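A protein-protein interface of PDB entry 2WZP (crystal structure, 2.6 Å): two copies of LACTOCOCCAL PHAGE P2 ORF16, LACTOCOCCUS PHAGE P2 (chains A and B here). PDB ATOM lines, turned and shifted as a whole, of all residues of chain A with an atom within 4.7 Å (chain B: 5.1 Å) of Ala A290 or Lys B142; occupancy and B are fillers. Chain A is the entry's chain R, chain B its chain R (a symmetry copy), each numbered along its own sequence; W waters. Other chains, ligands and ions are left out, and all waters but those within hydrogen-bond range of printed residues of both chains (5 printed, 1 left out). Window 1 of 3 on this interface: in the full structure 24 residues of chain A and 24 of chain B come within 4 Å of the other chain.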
ATOM      1  N   TYR A 241      15.528 -16.253  33.742  1.00  0.00           N
ATOM      2  CA  TYR A 241      15.813 -15.638  32.457  1.00  0.00           C
ATOM      3  C   TYR A 241      14.530 -15.494  31.707  1.00  0.00           C
ATOM      4  O   TYR A 241      13.690 -16.398  31.738  1.00  0.00           O
ATOM      5  CB  TYR A 241      16.797 -16.501  31.681  1.00  0.00           C
ATOM      6  CG  TYR A 241      18.133 -16.665  32.379  1.00  0.00           C
ATOM      7  CD1 TYR A 241      19.160 -15.745  32.189  1.00  0.00           C
ATOM      8  CD2 TYR A 241      18.387 -17.767  33.202  1.00  0.00           C
ATOM      9  CE1 TYR A 241      20.402 -15.913  32.800  1.00  0.00           C
ATOM     10  CE2 TYR A 241      19.616 -17.924  33.846  1.00  0.00           C
ATOM     11  CZ  TYR A 241      20.615 -16.987  33.655  1.00  0.00           C
ATOM     12  OH  TYR A 241      21.822 -17.119  34.309  1.00  0.00           O
ATOM     13  N   PHE A 243      14.553 -14.245  28.292  1.00  0.00           N
ATOM     14  CA  PHE A 243      14.958 -14.108  26.901  1.00  0.00           C
ATOM     15  C   PHE A 243      16.080 -15.105  26.617  1.00  0.00           C
ATOM     16  O   PHE A 243      16.928 -15.333  27.481  1.00  0.00           O
ATOM     17  CB  PHE A 243      15.431 -12.658  26.694  1.00  0.00           C
ATOM     18  CG  PHE A 243      15.691 -12.210  25.281  1.00  0.00           C
ATOM     19  CD1 PHE A 243      16.908 -12.483  24.660  1.00  0.00           C
ATOM     20  CD2 PHE A 243      14.786 -11.386  24.618  1.00  0.00           C
ATOM     21  CE1 PHE A 243      17.171 -12.016  23.367  1.00  0.00           C
ATOM     22  CE2 PHE A 243      15.052 -10.924  23.334  1.00  0.00           C
ATOM     23  CZ  PHE A 243      16.236 -11.253  22.707  1.00  0.00           C
ATOM     24  N   VAL A 245      19.038 -16.691  23.637  1.00  0.00           N
ATOM     25  CA  VAL A 245      19.847 -16.598  22.430  1.00  0.00           C
ATOM     26  C   VAL A 245      20.099 -18.061  22.128  1.00  0.00           C
ATOM     27  O   VAL A 245      20.703 -18.763  22.961  1.00  0.00           O
ATOM     28  CB  VAL A 245      21.148 -15.804  22.712  1.00  0.00           C
ATOM     29  CG1 VAL A 245      22.159 -15.930  21.570  1.00  0.00           C
ATOM     30  CG2 VAL A 245      20.820 -14.348  23.034  1.00  0.00           C
ATOM     31  N   PRO A 260      22.608 -17.344  15.809  1.00  0.00           N
ATOM     32  CA  PRO A 260      21.560 -17.721  16.761  1.00  0.00           C
ATOM     33  C   PRO A 260      20.223 -17.108  16.389  1.00  0.00           C
ATOM     34  O   PRO A 260      20.196 -16.144  15.626  1.00  0.00           O
ATOM     35  CB  PRO A 260      22.049 -17.113  18.083  1.00  0.00           C
ATOM     36  CG  PRO A 260      22.894 -15.961  17.691  1.00  0.00           C
ATOM     37  CD  PRO A 260      23.544 -16.351  16.389  1.00  0.00           C
ATOM     38  N   MET A 262      16.669 -15.683  18.467  1.00  0.00           N
ATOM     39  CA  MET A 262      16.315 -15.129  19.772  1.00  0.00           C
ATOM     40  C   MET A 262      14.866 -15.338  20.065  1.00  0.00           C
ATOM     41  O   MET A 262      14.026 -15.194  19.168  1.00  0.00           O
ATOM     42  CB  MET A 262      16.642 -13.622  19.825  1.00  0.00           C
ATOM     43  CG  MET A 262      18.078 -13.315  20.160  1.00  0.00           C
ATOM     44  SD  MET A 262      19.393 -13.969  19.078  1.00  0.00           S
ATOM     45  CE  MET A 262      19.063 -13.074  17.580  1.00  0.00           C
ATOM     46  N   ARG A 288      15.524  -7.000  30.484  1.00  0.00           N
ATOM     47  CA  ARG A 288      15.831  -8.231  29.746  1.00  0.00           C
ATOM     48  C   ARG A 288      16.909  -9.035  30.490  1.00  0.00           C
ATOM     49  O   ARG A 288      17.917  -8.477  30.916  1.00  0.00           O
ATOM     50  CB  ARG A 288      16.291  -7.919  28.322  1.00  0.00           C
ATOM     51  CG  ARG A 288      16.649  -9.169  27.521  1.00  0.00           C
ATOM     52  CD  ARG A 288      17.083  -8.832  26.133  1.00  0.00           C
ATOM     53  NE  ARG A 288      15.977  -8.274  25.349  1.00  0.00           N
ATOM     54  CZ  ARG A 288      16.144  -7.689  24.174  1.00  0.00           C
ATOM     55  NH1 ARG A 288      17.360  -7.564  23.652  1.00  0.00           N
ATOM     56  NH2 ARG A 288      15.110  -7.179  23.533  1.00  0.00           N
ATOM     57  N   THR A 289      16.694 -10.346  30.643  1.00  0.00           N
ATOM     58  CA  THR A 289      17.604 -11.281  31.340  1.00  0.00           C
ATOM     59  C   THR A 289      17.856 -12.456  30.381  1.00  0.00           C
ATOM     60  O   THR A 289      17.131 -13.443  30.390  1.00  0.00           O
ATOM     61  CB  THR A 289      17.022 -11.645  32.695  1.00  0.00           C
ATOM     62  OG1 THR A 289      15.678 -12.012  32.483  1.00  0.00           O
ATOM     63  CG2 THR A 289      17.014 -10.471  33.675  1.00  0.00           C
ATOM     64  N   ALA A 290      18.786 -12.258  29.439  1.00  0.00           N
ATOM     65  CA  ALA A 290      19.089 -13.231  28.394  1.00  0.00           C
ATOM     66  C   ALA A 290      19.999 -14.349  28.840  1.00  0.00           C
ATOM     67  O   ALA A 290      20.848 -14.166  29.736  1.00  0.00           O
ATOM     68  CB  ALA A 290      19.703 -12.529  27.187  1.00  0.00           C
ATOM     69  N   LYS A 291      19.837 -15.517  28.183  1.00  0.00           N
ATOM     70  CA  LYS A 291      20.700 -16.676  28.385  1.00  0.00           C
ATOM     71  C   LYS A 291      20.998 -17.308  27.032  1.00  0.00           C
ATOM     72  O   LYS A 291      20.188 -17.202  26.094  1.00  0.00           O
ATOM     73  CB  LYS A 291      20.127 -17.674  29.369  1.00  0.00           C
ATOM     74  CG  LYS A 291      19.100 -18.628  28.809  1.00  0.00           C
ATOM     75  CD  LYS A 291      18.253 -19.288  29.874  1.00  0.00           C
ATOM     76  CE  LYS A 291      18.924 -20.418  30.616  1.00  0.00           C
ATOM     77  NZ  LYS A 291      17.924 -21.326  31.284  1.00  0.00           N
ATOM     78  N   THR A 292      22.196 -17.903  26.908  1.00  0.00           N
ATOM     79  CA  THR A 292      22.589 -18.531  25.663  1.00  0.00           C
ATOM     80  C   THR A 292      22.335 -19.978  25.792  1.00  0.00           C
ATOM     81  O   THR A 292      22.617 -20.540  26.851  1.00  0.00           O
ATOM     82  CB  THR A 292      23.988 -18.120  25.203  1.00  0.00           C
ATOM     83  OG1 THR A 292      24.097 -16.713  25.318  1.00  0.00           O
ATOM     84  CG2 THR A 292      24.233 -18.462  23.788  1.00  0.00           C
ATOM     85  N   GLU B 117      26.399  -9.234  29.711  1.00  0.00           N
ATOM     86  CA  GLU B 117      26.252 -10.259  30.751  1.00  0.00           C
ATOM     87  C   GLU B 117      25.431 -11.423  30.191  1.00  0.00           C
ATOM     88  O   GLU B 117      24.446 -11.186  29.478  1.00  0.00           O
ATOM     89  CB  GLU B 117      25.483  -9.702  31.970  1.00  0.00           C
ATOM     90  CG  GLU B 117      26.328  -8.952  32.975  1.00  0.00           C
ATOM     91  CD  GLU B 117      25.558  -8.292  34.103  1.00  0.00           C
ATOM     92  OE1 GLU B 117      24.320  -8.149  33.983  1.00  0.00           O
ATOM     93  OE2 GLU B 117      26.197  -7.919  35.114  1.00  0.00           O
ATOM     94  N   SER B 118      25.811 -12.667  30.558  1.00  0.00           N
ATOM     95  CA  SER B 118      25.132 -13.922  30.222  1.00  0.00           C
ATOM     96  C   SER B 118      25.166 -14.365  28.781  1.00  0.00           C
ATOM     97  O   SER B 118      24.669 -15.461  28.501  1.00  0.00           O
ATOM     98  CB  SER B 118      23.708 -13.945  30.758  1.00  0.00           C
ATOM     99  OG  SER B 118      23.639 -13.626  32.139  1.00  0.00           O
ATOM    100  N   LEU B 119      25.763 -13.555  27.863  1.00  0.00           N
ATOM    101  CA  LEU B 119      25.929 -13.919  26.448  1.00  0.00           C
ATOM    102  C   LEU B 119      27.158 -14.846  26.326  1.00  0.00           C
ATOM    103  O   LEU B 119      28.212 -14.549  26.899  1.00  0.00           O
ATOM    104  CB  LEU B 119      26.126 -12.645  25.584  1.00  0.00           C
ATOM    105  CG  LEU B 119      26.226 -12.858  24.064  1.00  0.00           C
ATOM    106  CD1 LEU B 119      24.930 -13.287  23.473  1.00  0.00           C
ATOM    107  CD2 LEU B 119      26.786 -11.641  23.372  1.00  0.00           C
ATOM    108  N   ASP B 135      30.782  -7.119  16.465  1.00  0.00           N
ATOM    109  CA  ASP B 135      29.454  -7.019  15.883  1.00  0.00           C
ATOM    110  C   ASP B 135      28.488  -8.073  16.462  1.00  0.00           C
ATOM    111  O   ASP B 135      27.284  -7.815  16.569  1.00  0.00           O
ATOM    112  CB  ASP B 135      29.609  -7.122  14.367  1.00  0.00           C
ATOM    113  CG  ASP B 135      28.359  -6.898  13.552  1.00  0.00           C
ATOM    114  OD1 ASP B 135      27.727  -5.817  13.705  1.00  0.00           O
ATOM    115  OD2 ASP B 135      28.048  -7.765  12.705  1.00  0.00           O
ATOM    116  N   TYR B 136      29.008  -9.238  16.881  1.00  0.00           N
ATOM    117  CA  TYR B 136      28.194 -10.283  17.511  1.00  0.00           C
ATOM    118  C   TYR B 136      27.847  -9.832  18.948  1.00  0.00           C
ATOM    119  O   TYR B 136      26.690  -9.898  19.381  1.00  0.00           O
ATOM    120  CB  TYR B 136      28.916 -11.646  17.486  1.00  0.00           C
ATOM    121  CG  TYR B 136      28.261 -12.687  18.372  1.00  0.00           C
ATOM    122  CD1 TYR B 136      27.047 -13.274  18.019  1.00  0.00           C
ATOM    123  CD2 TYR B 136      28.798 -13.007  19.618  1.00  0.00           C
ATOM    124  CE1 TYR B 136      26.409 -14.183  18.863  1.00  0.00           C
ATOM    125  CE2 TYR B 136      28.160 -13.906  20.472  1.00  0.00           C
ATOM    126  CZ  TYR B 136      26.976 -14.501  20.082  1.00  0.00           C
ATOM    127  OH  TYR B 136      26.357 -15.376  20.925  1.00  0.00           O
ATOM    128  N   ASP B 139      24.699  -5.786  20.163  1.00  0.00           N
ATOM    129  CA  ASP B 139      23.454  -6.058  19.463  1.00  0.00           C
ATOM    130  C   ASP B 139      22.238  -5.929  20.408  1.00  0.00           C
ATOM    131  O   ASP B 139      22.013  -6.827  21.246  1.00  0.00           O
ATOM    132  CB  ASP B 139      23.505  -7.501  18.890  1.00  0.00           C
ATOM    133  CG  ASP B 139      22.328  -7.862  18.024  1.00  0.00           C
ATOM    134  OD1 ASP B 139      21.608  -6.931  17.570  1.00  0.00           O
ATOM    135  OD2 ASP B 139      22.122  -9.067  17.791  1.00  0.00           O
ATOM    136  N   PRO B 140      21.370  -4.901  20.193  1.00  0.00           N
ATOM    137  CA  PRO B 140      20.164  -4.751  21.039  1.00  0.00           C
ATOM    138  C   PRO B 140      19.139  -5.876  20.872  1.00  0.00           C
ATOM    139  O   PRO B 140      18.209  -6.002  21.666  1.00  0.00           O
ATOM    140  CB  PRO B 140      19.610  -3.405  20.591  1.00  0.00           C
ATOM    141  CG  PRO B 140      20.103  -3.232  19.190  1.00  0.00           C
ATOM    142  CD  PRO B 140      21.470  -3.803  19.205  1.00  0.00           C
ATOM    143  N   ASN B 141      19.309  -6.706  19.833  1.00  0.00           N
ATOM    144  CA  ASN B 141      18.426  -7.852  19.597  1.00  0.00           C
ATOM    145  C   ASN B 141      18.820  -9.009  20.484  1.00  0.00           C
ATOM    146  O   ASN B 141      18.062  -9.953  20.546  1.00  0.00           O
ATOM    147  CB  ASN B 141      18.490  -8.304  18.136  1.00  0.00           C
ATOM    148  CG  ASN B 141      17.979  -7.295  17.179  1.00  0.00           C
ATOM    149  OD1 ASN B 141      16.793  -7.029  17.096  1.00  0.00           O
ATOM    150  ND2 ASN B 141      18.863  -6.679  16.459  1.00  0.00           N
ATOM    151  N   LYS B 142      19.992  -8.967  21.141  1.00  0.00           N
ATOM    152  CA  LYS B 142      20.459 -10.038  22.049  1.00  0.00           C
ATOM    153  C   LYS B 142      20.780  -9.504  23.449  1.00  0.00           C
ATOM    154  O   LYS B 142      20.610 -10.232  24.421  1.00  0.00           O
ATOM    155  CB  LYS B 142      21.775 -10.698  21.554  1.00  0.00           C
ATOM    156  CG  LYS B 142      21.697 -11.452  20.245  1.00  0.00           C
ATOM    157  CD  LYS B 142      22.960 -12.302  20.012  1.00  0.00           C
ATOM    158  CE  LYS B 142      24.184 -11.529  19.649  1.00  0.00           C
ATOM    159  NZ  LYS B 142      24.189 -11.092  18.235  1.00  0.00           N
ATOM    160  N   ASN B 143      21.391  -8.308  23.541  1.00  0.00           N
ATOM    161  CA  ASN B 143      21.875  -7.778  24.827  1.00  0.00           C
ATOM    162  C   ASN B 143      20.805  -7.449  25.810  1.00  0.00           C
ATOM    163  O   ASN B 143      19.682  -7.175  25.430  1.00  0.00           O
ATOM    164  CB  ASN B 143      22.787  -6.565  24.634  1.00  0.00           C
ATOM    165  CG  ASN B 143      23.964  -6.800  23.763  1.00  0.00           C
ATOM    166  OD1 ASN B 143      24.501  -7.908  23.669  1.00  0.00           O
ATOM    167  ND2 ASN B 143      24.398  -5.756  23.136  1.00  0.00           N
ATOM    168  N   ASN B 144      21.187  -7.469  27.087  1.00  0.00           N
ATOM    169  CA  ASN B 144      20.371  -7.163  28.250  1.00  0.00           C
ATOM    170  C   ASN B 144      20.108  -5.666  28.339  1.00  0.00           C
ATOM    171  O   ASN B 144      19.079  -5.263  28.897  1.00  0.00           O
ATOM    172  CB  ASN B 144      21.088  -7.656  29.521  1.00  0.00           C
ATOM    173  CG  ASN B 144      20.859  -9.109  29.821  1.00  0.00           C
ATOM    174  OD1 ASN B 144      20.107  -9.799  29.132  1.00  0.00           O
ATOM    175  ND2 ASN B 144      21.469  -9.598  30.884  1.00  0.00           N
HETATM  176  O   HOH W   1      24.006 -17.820  29.295  1.00  0.00           O
HETATM  177  O   HOH W   2      17.271  -4.820  30.717  1.00  0.00           O
HETATM  178  O   HOH W   3      24.245 -15.636  33.826  1.00  0.00           O
HETATM  179  O   HOH W   4      22.593 -14.633  26.767  1.00  0.00           O
HETATM  180  O   HOH W   5      21.330 -12.409  31.922  1.00  0.00           O
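Water W1 bridges O of Ser B118 and N of Thr A292.
Water W2 lies within hydrogen-bond range of O of Asn B144 and N of Arg A288.
Water W5 lies within hydrogen-bond range of the side-chain hydroxyl (OG) of Ser B118, the backbone carbonyl oxygen (O) of Ala A290 and the side-chain amide nitrogen (ND2) of Asn B144.
Water W3 bridges the side-chain hydroxyl of Ser B118 and the side-chain hydroxyl of Tyr A241.
Water W4 lies within hydrogen-bond range of O of Ser B118 (2.8 Å), OG1 of Thr A292 (2.9 Å), N of Lys A291 (3.2 Å) and O of Ala A290 (3.5 Å).
Ala A290 touches three residues of chain B.
Of the printed residues of chain A, Lys B142 touches Met A262 (3.6 Å), Arg A288 (3.9 Å) and Ala A290 (3.7 Å).
Of the printed residues of chain A, Ser B118 touches Ala A290 and Thr A292.
Printed residues of chain A within 4 Å of Asn B141: Phe A243 (3.1 Å), Met A262 (3.4 Å) and Arg A288 (3.8 Å).
Of the printed residues of chain A, Asn B144 touches Arg A288 (3.1 Å), Thr A289 (3.7 Å) and Ala A290 (2.8 Å).
Of the printed residues of chain B, Thr A289 touches Asn B144.
Printed residues of chain B within 4 Å of Arg A288: Pro B140, Asn B141, Lys B142, Asn B143 and Asn B144.
Asp B135 touches none of the printed residues of chain A.
The nearest printed residue of chain A that does not touch Lys B142 is Phe A243 (4.02 Å).
The nearest printed residue of chain B that does not touch Phe A243 is Lys B142 (4.02 Å).
Among the printed residues, merely in contact across the chains: Phe A243 with Asn B141 (3.1 Å), Met A262 with Asn B141 (3.4 Å), Met A262 with Lys B142 (3.6 Å), Arg A288 with Asn B141 (3.8 Å), Arg A288 with Lys B142 (3.9 Å), Thr A289 with Asn B144 (3.7 Å), Ala A290 with Ser B118 (3.0 Å), Ala A290 with Lys B142 (3.7 Å) and Thr A292 with Leu B119 (3.5 Å).
The guanidinium group (NH1) of Arg A288 is in hydrogen-bond range of the backbone carbonyl oxygen (O) of Pro B140 (2.7 Å).
The guanidinium group (NH1) of Arg A288 lies within hydrogen-bond range of the backbone carbonyl oxygen (O) of Asn B143, 3.0 Å away.
OD1 of Asn B144 sits close to O of Arg A288, at 3.1 Å.
The backbone NH (N) of Ala A290 lies within hydrogen-bond range of the side-chain amide oxygen (OD1) of Asn B144 (2.8 Å).
OG1 of Thr A292 sits at hydrogen-bond distance from O of Ser B118, 3.5 Å away.
No position is printed for both chains.
N of Phe A243 is in hydrogen-bond range of O of Thr A289 (3.4 Å).
The backbone NH (N) of Lys A291 is in hydrogen-bond range of the backbone carbonyl oxygen (O) of Phe A243 (3.0 Å).
The side-chain amino group (NZ) of Lys B142 sits at hydrogen-bond distance from the backbone carbonyl oxygen (O) of Tyr B136 (3.0 Å).
The side-chain amide nitrogen (ND2) of Asn B141 sits at hydrogen-bond distance from the side-chain carboxylate (OD1) of Asp B139.
NZ of Lys B142 is in salt-bridge range of OD2 of Asp B139 (2.9 Å).
N of Asp B139 lies close to ND2 of Asn B143 (3.0 Å).
Of the 11 printed residues of chain B, 7 touch a printed residue of chain A.
Hydrophobic or aromatic side chains of chain B that line the printed part of chain A: Leu B119.
Of the 10 printed residues of chain A, 6 touch a printed residue of chain B.
Hydrophobic or aromatic side chains of chain A within 4 Å of the printed part of chain B: Phe A243, Met A262 and Ala A290.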
